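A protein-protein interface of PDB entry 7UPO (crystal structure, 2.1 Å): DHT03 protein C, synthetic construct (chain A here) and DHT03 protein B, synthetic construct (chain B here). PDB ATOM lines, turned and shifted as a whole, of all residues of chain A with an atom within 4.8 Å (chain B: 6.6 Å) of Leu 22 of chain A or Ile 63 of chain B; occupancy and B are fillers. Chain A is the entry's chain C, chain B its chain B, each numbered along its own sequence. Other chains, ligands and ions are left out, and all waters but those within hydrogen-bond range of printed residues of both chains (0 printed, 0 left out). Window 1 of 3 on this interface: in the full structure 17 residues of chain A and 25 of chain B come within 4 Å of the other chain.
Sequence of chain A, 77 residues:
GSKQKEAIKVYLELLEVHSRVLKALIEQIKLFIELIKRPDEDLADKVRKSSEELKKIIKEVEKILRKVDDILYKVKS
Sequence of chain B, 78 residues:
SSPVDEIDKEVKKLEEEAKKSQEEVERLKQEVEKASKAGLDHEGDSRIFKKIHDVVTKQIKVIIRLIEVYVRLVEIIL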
ATOM      1  N   HIS A  18     -20.747  12.328  14.765  1.00  0.00           N
ATOM      2  CA  HIS A  18     -20.951  13.323  13.716  1.00  0.00           C
ATOM      3  C   HIS A  18     -22.400  13.780  13.635  1.00  0.00           C
ATOM      4  O   HIS A  18     -22.666  14.901  13.188  1.00  0.00           O
ATOM      5  CB  HIS A  18     -20.488  12.767  12.370  1.00  0.00           C
ATOM      6  CG  HIS A  18     -19.000  12.733  12.214  1.00  0.00           C
ATOM      7  ND1 HIS A  18     -18.378  12.171  11.121  1.00  0.00           N
ATOM      8  CD2 HIS A  18     -18.010  13.196  13.015  1.00  0.00           C
ATOM      9  CE1 HIS A  18     -17.069  12.287  11.256  1.00  0.00           C
ATOM     10  NE2 HIS A  18     -16.820  12.906  12.395  1.00  0.00           N
ATOM     11  N   SER A  19     -23.347  12.936  14.052  1.00  0.00           N
ATOM     12  CA  SER A  19     -24.734  13.381  14.131  1.00  0.00           C
ATOM     13  C   SER A  19     -24.874  14.547  15.097  1.00  0.00           C
ATOM     14  O   SER A  19     -25.564  15.531  14.804  1.00  0.00           O
ATOM     15  CB  SER A  19     -25.638  12.225  14.555  1.00  0.00           C
ATOM     16  OG  SER A  19     -25.727  11.245  13.534  1.00  0.00           O
ATOM     17  N   ARG A  20     -24.213  14.461  16.254  1.00  0.00           N
ATOM     18  CA  ARG A  20     -24.252  15.551  17.218  1.00  0.00           C
ATOM     19  C   ARG A  20     -23.422  16.745  16.769  1.00  0.00           C
ATOM     20  O   ARG A  20     -23.672  17.864  17.230  1.00  0.00           O
ATOM     21  CB  ARG A  20     -23.787  15.048  18.588  1.00  0.00           C
ATOM     22  CG  ARG A  20     -24.709  13.988  19.174  1.00  0.00           C
ATOM     23  CD  ARG A  20     -24.363  13.629  20.611  1.00  0.00           C
ATOM     24  NE  ARG A  20     -23.290  12.645  20.697  1.00  0.00           N
ATOM     25  CZ  ARG A  20     -22.048  12.928  21.071  1.00  0.00           C
ATOM     26  NH1 ARG A  20     -21.720  14.170  21.399  1.00  0.00           N
ATOM     27  NH2 ARG A  20     -21.134  11.969  21.124  1.00  0.00           N
ATOM     28  N   VAL A  21     -22.447  16.538  15.880  1.00  0.00           N
ATOM     29  CA  VAL A  21     -21.733  17.670  15.296  1.00  0.00           C
ATOM     30  C   VAL A  21     -22.630  18.406  14.310  1.00  0.00           C
ATOM     31  O   VAL A  21     -22.665  19.643  14.283  1.00  0.00           O
ATOM     32  CB  VAL A  21     -20.428  17.200  14.631  1.00  0.00           C
ATOM     33  CG1 VAL A  21     -19.706  18.374  13.990  1.00  0.00           C
ATOM     34  CG2 VAL A  21     -19.533  16.523  15.648  1.00  0.00           C
ATOM     35  N   LEU A  22     -23.364  17.661  13.482  1.00  0.00           N
ATOM     36  CA  LEU A  22     -24.333  18.277  12.580  1.00  0.00           C
ATOM     37  C   LEU A  22     -25.358  19.092  13.356  1.00  0.00           C
ATOM     38  O   LEU A  22     -25.612  20.259  13.037  1.00  0.00           O
ATOM     39  CB  LEU A  22     -25.027  17.200  11.745  1.00  0.00           C
ATOM     40  CG  LEU A  22     -24.260  16.617  10.559  1.00  0.00           C
ATOM     41  CD1 LEU A  22     -24.853  15.280  10.147  1.00  0.00           C
ATOM     42  CD2 LEU A  22     -24.293  17.591   9.397  1.00  0.00           C
ATOM     43  N   LYS A  23     -25.951  18.490  14.390  1.00  0.00           N
ATOM     44  CA  LYS A  23     -26.973  19.179  15.172  1.00  0.00           C
ATOM     45  C   LYS A  23     -26.417  20.436  15.829  1.00  0.00           C
ATOM     46  O   LYS A  23     -27.083  21.478  15.853  1.00  0.00           O
ATOM     47  CB  LYS A  23     -27.546  18.229  16.225  1.00  0.00           C
ATOM     48  CG  LYS A  23     -28.640  18.826  17.088  1.00  0.00           C
ATOM     49  CD  LYS A  23     -29.150  17.802  18.089  1.00  0.00           C
ATOM     50  CE  LYS A  23     -30.308  18.344  18.908  1.00  0.00           C
ATOM     51  NZ  LYS A  23     -30.842  17.316  19.844  1.00  0.00           N
ATOM     52  N   ALA A  24     -25.193  20.362  16.358  1.00  0.00           N
ATOM     53  CA  ALA A  24     -24.608  21.523  17.022  1.00  0.00           C
ATOM     54  C   ALA A  24     -24.220  22.600  16.018  1.00  0.00           C
ATOM     55  O   ALA A  24     -24.398  23.796  16.280  1.00  0.00           O
ATOM     56  CB  ALA A  24     -23.396  21.100  17.851  1.00  0.00           C
ATOM     57  N   LEU A  25     -23.689  22.197  14.862  1.00  0.00           N
ATOM     58  CA  LEU A  25     -23.240  23.174  13.876  1.00  0.00           C
ATOM     59  C   LEU A  25     -24.420  23.909  13.250  1.00  0.00           C
ATOM     60  O   LEU A  25     -24.334  25.110  12.972  1.00  0.00           O
ATOM     61  CB  LEU A  25     -22.401  22.481  12.803  1.00  0.00           C
ATOM     62  CG  LEU A  25     -21.405  23.342  12.031  1.00  0.00           C
ATOM     63  CD1 LEU A  25     -20.441  24.023  12.988  1.00  0.00           C
ATOM     64  CD2 LEU A  25     -20.644  22.491  11.029  1.00  0.00           C
ATOM     65  N   ILE A  26     -25.532  23.206  13.022  1.00  0.00           N
ATOM     66  CA  ILE A  26     -26.717  23.854  12.470  1.00  0.00           C
ATOM     67  C   ILE A  26     -27.274  24.876  13.452  1.00  0.00           C
ATOM     68  O   ILE A  26     -27.684  25.974  13.058  1.00  0.00           O
ATOM     69  CB  ILE A  26     -27.772  22.802  12.085  1.00  0.00           C
ATOM     70  CG1 ILE A  26     -27.285  21.962  10.901  1.00  0.00           C
ATOM     71  CG2 ILE A  26     -29.098  23.468  11.752  1.00  0.00           C
ATOM     72  CD1 ILE A  26     -28.211  20.820  10.540  1.00  0.00           C
ATOM     73  N   LEU B  14     -29.515  22.213   3.710  1.00  0.00           N
ATOM     74  CA  LEU B  14     -28.554  21.298   4.318  1.00  0.00           C
ATOM     75  C   LEU B  14     -29.125  20.629   5.560  1.00  0.00           C
ATOM     76  O   LEU B  14     -28.770  19.484   5.863  1.00  0.00           O
ATOM     77  CB  LEU B  14     -27.263  22.039   4.663  1.00  0.00           C
ATOM     78  CG  LEU B  14     -26.439  22.523   3.469  1.00  0.00           C
ATOM     79  CD1 LEU B  14     -25.216  23.286   3.938  1.00  0.00           C
ATOM     80  CD2 LEU B  14     -26.037  21.345   2.597  1.00  0.00           C
ATOM     81  N   GLU B  17     -30.899  17.660   4.424  1.00  0.00           N
ATOM     82  CA  GLU B  17     -29.953  16.604   4.083  1.00  0.00           C
ATOM     83  C   GLU B  17     -29.440  15.904   5.332  1.00  0.00           C
ATOM     84  O   GLU B  17     -29.185  14.695   5.304  1.00  0.00           O
ATOM     85  CB  GLU B  17     -28.783  17.172   3.280  1.00  0.00           C
ATOM     86  CG  GLU B  17     -29.164  17.738   1.924  1.00  0.00           C
ATOM     87  CD  GLU B  17     -27.954  18.120   1.094  1.00  0.00           C
ATOM     88  OE1 GLU B  17     -26.829  17.734   1.475  1.00  0.00           O
ATOM     89  OE2 GLU B  17     -28.125  18.805   0.064  1.00  0.00           O
ATOM     90  N   ALA B  18     -29.288  16.644   6.431  1.00  0.00           N
ATOM     91  CA  ALA B  18     -28.900  16.026   7.693  1.00  0.00           C
ATOM     92  C   ALA B  18     -29.967  15.048   8.169  1.00  0.00           C
ATOM     93  O   ALA B  18     -29.656  13.935   8.607  1.00  0.00           O
ATOM     94  CB  ALA B  18     -28.648  17.103   8.749  1.00  0.00           C
ATOM     95  N   SER B  21     -29.701  12.082   6.083  1.00  0.00           N
ATOM     96  CA  SER B  21     -28.509  11.339   6.471  1.00  0.00           C
ATOM     97  C   SER B  21     -28.777  10.503   7.714  1.00  0.00           C
ATOM     98  O   SER B  21     -28.457   9.309   7.754  1.00  0.00           O
ATOM     99  CB  SER B  21     -27.344  12.297   6.710  1.00  0.00           C
ATOM    100  OG  SER B  21     -26.266  11.629   7.345  1.00  0.00           O
ATOM    101  N   GLN B  22     -29.377  11.116   8.738  1.00  0.00           N
ATOM    102  CA  GLN B  22     -29.673  10.385   9.965  1.00  0.00           C
ATOM    103  C   GLN B  22     -30.602   9.211   9.693  1.00  0.00           C
ATOM    104  O   GLN B  22     -30.456   8.143  10.297  1.00  0.00           O
ATOM    105  CB  GLN B  22     -30.285  11.324  11.001  1.00  0.00           C
ATOM    106  CG  GLN B  22     -30.366  10.720  12.389  1.00  0.00           C
ATOM    107  CD  GLN B  22     -29.005  10.296  12.909  1.00  0.00           C
ATOM    108  OE1 GLN B  22     -28.039  11.053  12.835  1.00  0.00           O
ATOM    109  NE2 GLN B  22     -28.920   9.077  13.427  1.00  0.00           N
ATOM    110  N   LYS B  58     -20.491  10.203   3.229  1.00  0.00           N
ATOM    111  CA  LYS B  58     -21.603  11.093   2.903  1.00  0.00           C
ATOM    112  C   LYS B  58     -21.885  12.062   4.043  1.00  0.00           C
ATOM    113  O   LYS B  58     -22.108  13.256   3.814  1.00  0.00           O
ATOM    114  CB  LYS B  58     -22.859  10.281   2.583  1.00  0.00           C
ATOM    115  CG  LYS B  58     -22.859   9.600   1.227  1.00  0.00           C
ATOM    116  CD  LYS B  58     -24.212   8.954   0.957  1.00  0.00           C
ATOM    117  CE  LYS B  58     -24.279   8.344  -0.432  1.00  0.00           C
ATOM    118  NZ  LYS B  58     -25.637   7.804  -0.731  1.00  0.00           N
ATOM    119  N   GLN B  59     -21.868  11.565   5.281  1.00  0.00           N
ATOM    120  CA  GLN B  59     -22.203  12.404   6.426  1.00  0.00           C
ATOM    121  C   GLN B  59     -21.181  13.519   6.615  1.00  0.00           C
ATOM    122  O   GLN B  59     -21.550  14.662   6.909  1.00  0.00           O
ATOM    123  CB  GLN B  59     -22.301  11.542   7.683  1.00  0.00           C
ATOM    124  CG  GLN B  59     -22.877  12.253   8.891  1.00  0.00           C
ATOM    125  CD  GLN B  59     -22.814  11.395  10.138  1.00  0.00           C
ATOM    126  OE1 GLN B  59     -21.857  10.646  10.341  1.00  0.00           O
ATOM    127  NE2 GLN B  59     -23.839  11.493  10.977  1.00  0.00           N
ATOM    128  N   ILE B  60     -19.895  13.206   6.449  1.00  0.00           N
ATOM    129  CA  ILE B  60     -18.857  14.224   6.586  1.00  0.00           C
ATOM    130  C   ILE B  60     -18.977  15.262   5.477  1.00  0.00           C
ATOM    131  O   ILE B  60     -18.760  16.459   5.702  1.00  0.00           O
ATOM    132  CB  ILE B  60     -17.465  13.565   6.603  1.00  0.00           C
ATOM    133  CG1 ILE B  60     -17.317  12.669   7.832  1.00  0.00           C
ATOM    134  CG2 ILE B  60     -16.371  14.615   6.577  1.00  0.00           C
ATOM    135  CD1 ILE B  60     -16.003  11.919   7.886  1.00  0.00           C
ATOM    136  N   LYS B  61     -19.330  14.825   4.266  1.00  0.00           N
ATOM    137  CA  LYS B  61     -19.517  15.767   3.169  1.00  0.00           C
ATOM    138  C   LYS B  61     -20.667  16.726   3.447  1.00  0.00           C
ATOM    139  O   LYS B  61     -20.626  17.885   3.018  1.00  0.00           O
ATOM    140  CB  LYS B  61     -19.749  15.011   1.861  1.00  0.00           C
ATOM    141  CG  LYS B  61     -18.497  14.366   1.286  1.00  0.00           C
ATOM    142  CD  LYS B  61     -18.800  13.630  -0.008  1.00  0.00           C
ATOM    143  CE  LYS B  61     -17.535  13.066  -0.632  1.00  0.00           C
ATOM    144  NZ  LYS B  61     -17.826  12.298  -1.873  1.00  0.00           N
ATOM    145  N   VAL B  62     -21.697  16.266   4.160  1.00  0.00           N
ATOM    146  CA  VAL B  62     -22.755  17.174   4.589  1.00  0.00           C
ATOM    147  C   VAL B  62     -22.210  18.185   5.589  1.00  0.00           C
ATOM    148  O   VAL B  62     -22.587  19.362   5.571  1.00  0.00           O
ATOM    149  CB  VAL B  62     -23.942  16.381   5.166  1.00  0.00           C
ATOM    150  CG1 VAL B  62     -25.013  17.325   5.694  1.00  0.00           C
ATOM    151  CG2 VAL B  62     -24.524  15.459   4.107  1.00  0.00           C
ATOM    152  N   ILE B  63     -21.304  17.745   6.466  1.00  0.00           N
ATOM    153  CA  ILE B  63     -20.691  18.654   7.431  1.00  0.00           C
ATOM    154  C   ILE B  63     -19.849  19.701   6.711  1.00  0.00           C
ATOM    155  O   ILE B  63     -19.891  20.892   7.042  1.00  0.00           O
ATOM    156  CB  ILE B  63     -19.849  17.869   8.452  1.00  0.00           C
ATOM    157  CG1 ILE B  63     -20.727  16.908   9.256  1.00  0.00           C
ATOM    158  CG2 ILE B  63     -19.110  18.825   9.371  1.00  0.00           C
ATOM    159  CD1 ILE B  63     -19.948  16.040  10.219  1.00  0.00           C
ATOM    160  N   ILE B  64     -19.070  19.266   5.718  1.00  0.00           N
ATOM    161  CA  ILE B  64     -18.196  20.185   4.991  1.00  0.00           C
ATOM    162  C   ILE B  64     -19.016  21.256   4.280  1.00  0.00           C
ATOM    163  O   ILE B  64     -18.669  22.444   4.306  1.00  0.00           O
ATOM    164  CB  ILE B  64     -17.305  19.402   4.010  1.00  0.00           C
ATOM    165  CG1 ILE B  64     -16.293  18.548   4.780  1.00  0.00           C
ATOM    166  CG2 ILE B  64     -16.601  20.349   3.046  1.00  0.00           C
ATOM    167  CD1 ILE B  64     -15.432  17.665   3.900  1.00  0.00           C
ATOM    168  N   ARG B  65     -20.117  20.858   3.638  1.00  0.00           N
ATOM    169  CA  ARG B  65     -20.974  21.841   2.982  1.00  0.00           C
ATOM    170  C   ARG B  65     -21.567  22.814   3.994  1.00  0.00           C
ATOM    171  O   ARG B  65     -21.712  24.007   3.705  1.00  0.00           O
ATOM    172  CB  ARG B  65     -22.076  21.139   2.191  1.00  0.00           C
ATOM    173  CG  ARG B  65     -21.564  20.360   0.988  1.00  0.00           C
ATOM    174  CD  ARG B  65     -22.685  20.028   0.014  1.00  0.00           C
ATOM    175  NE  ARG B  65     -23.708  19.179   0.615  1.00  0.00           N
ATOM    176  CZ  ARG B  65     -23.615  17.858   0.719  1.00  0.00           C
ATOM    177  NH1 ARG B  65     -22.540  17.228   0.265  1.00  0.00           N
ATOM    178  NH2 ARG B  65     -24.597  17.164   1.278  1.00  0.00           N
ATOM    179  N   LEU B  66     -21.902  22.324   5.192  1.00  0.00           N
ATOM    180  CA  LEU B  66     -22.357  23.216   6.254  1.00  0.00           C
ATOM    181  C   LEU B  66     -21.283  24.231   6.619  1.00  0.00           C
ATOM    182  O   LEU B  66     -21.575  25.420   6.797  1.00  0.00           O
ATOM    183  CB  LEU B  66     -22.758  22.408   7.487  1.00  0.00           C
ATOM    184  CG  LEU B  66     -24.227  22.021   7.638  1.00  0.00           C
ATOM    185  CD1 LEU B  66     -24.408  21.179   8.887  1.00  0.00           C
ATOM    186  CD2 LEU B  66     -25.104  23.264   7.695  1.00  0.00           C
ATOM    187  N   ILE B  67     -20.033  23.780   6.739  1.00  0.00           N
ATOM    188  CA  ILE B  67     -18.950  24.681   7.119  1.00  0.00           C
ATOM    189  C   ILE B  67     -18.689  25.698   6.016  1.00  0.00           C
ATOM    190  O   ILE B  67     -18.469  26.885   6.289  1.00  0.00           O
ATOM    191  CB  ILE B  67     -17.684  23.875   7.461  1.00  0.00           C
ATOM    192  CG1 ILE B  67     -17.951  22.949   8.650  1.00  0.00           C
ATOM    193  CG2 ILE B  67     -16.520  24.804   7.756  1.00  0.00           C
ATOM    194  CD1 ILE B  67     -16.792  22.045   8.998  1.00  0.00           C
ATOM    195  N   GLU B  68     -18.711  25.257   4.756  1.00  0.00           N
ATOM    196  CA  GLU B  68     -18.514  26.190   3.651  1.00  0.00           C
ATOM    197  C   GLU B  68     -19.625  27.228   3.596  1.00  0.00           C
ATOM    198  O   GLU B  68     -19.381  28.378   3.214  1.00  0.00           O
ATOM    199  CB  GLU B  68     -18.418  25.425   2.332  1.00  0.00           C
ATOM    200  CG  GLU B  68     -17.198  24.525   2.235  1.00  0.00           C
ATOM    201  CD  GLU B  68     -17.217  23.640   1.005  1.00  0.00           C
ATOM    202  OE1 GLU B  68     -18.293  23.504   0.388  1.00  0.00           O
ATOM    203  OE2 GLU B  68     -16.156  23.081   0.652  1.00  0.00           O
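Arg 20 of chain A touches none of the printed residues of chain B. Of chain B, only Gln 59 (3.8 Å), Val 62 (3.8 Å), Ile 63 (3.6 Å) and Leu 66 (3.6 Å) come within 4 Å of Leu 22 of chain A. Of the printed residues of chain B, Leu 25 of chain A touches Ile 67. Of the printed residues of chain A, Ile 60 of chain B touches His 18 (3.5 Å). Ile 63 of chain B touches two residues of chain A. Of the printed residues of chain A, Ile 67 of chain B touches Leu 25. The nearest residue of chain B that does not touch Leu 22 of chain A is Ala 18 of chain B (4.4 Å).
The side-chain hydroxyl (OG) of Ser 19 of chain A lies within hydrogen-bond range of the side-chain amide oxygen (OE1) of Gln 22 of chain B, 2.4 Å away. OG of Ser 19 of chain A lies within hydrogen-bond range of NE2 of Gln 59 of chain B, at 3.2 Å.
Gln 59 of chain B touches His 18 of chain A (OE1 to CB, 3.2 Å). Ile 60 of chain B touches His 18 of chain A. His 18 of chain A touches Ile 63 of chain B (CB to CD1, 3.95 Å). CG of Gln 59 of chain B touches CD1 of Leu 22 of chain A (3.8 Å). Leu 22 of chain A touches Val 62 of chain B (CD2 to CG1, 3.8 Å). Leu 22 of chain A touches Ile 63 of chain B (CD2 to CG1, 3.6 Å). Leu 22 of chain A touches Leu 66 of chain B (CD2 to CD1, 3.6 Å). Leu 25 of chain A touches Ile 67 of chain B. Ile 26 of chain A touches Leu 66 of chain B (CG1 to CD1, 3.6 Å).
Hydrophobic or aromatic side chains of chain B within 4 Å of the printed part of chain A: Ile 60, Val 62, Ile 63, Leu 66 and Ile 67. Hydrophobic or aromatic side chains of chain A within 4 Å of the printed part of chain B: His 18, Leu 22, Leu 25 and Ile 26. Among the printed residues, 11 pairs touch across the chains. Among the printed residues, no Asp or Glu carboxylate lies within 4 Å of a Lys or Arg side-chain nitrogen of the other chain.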
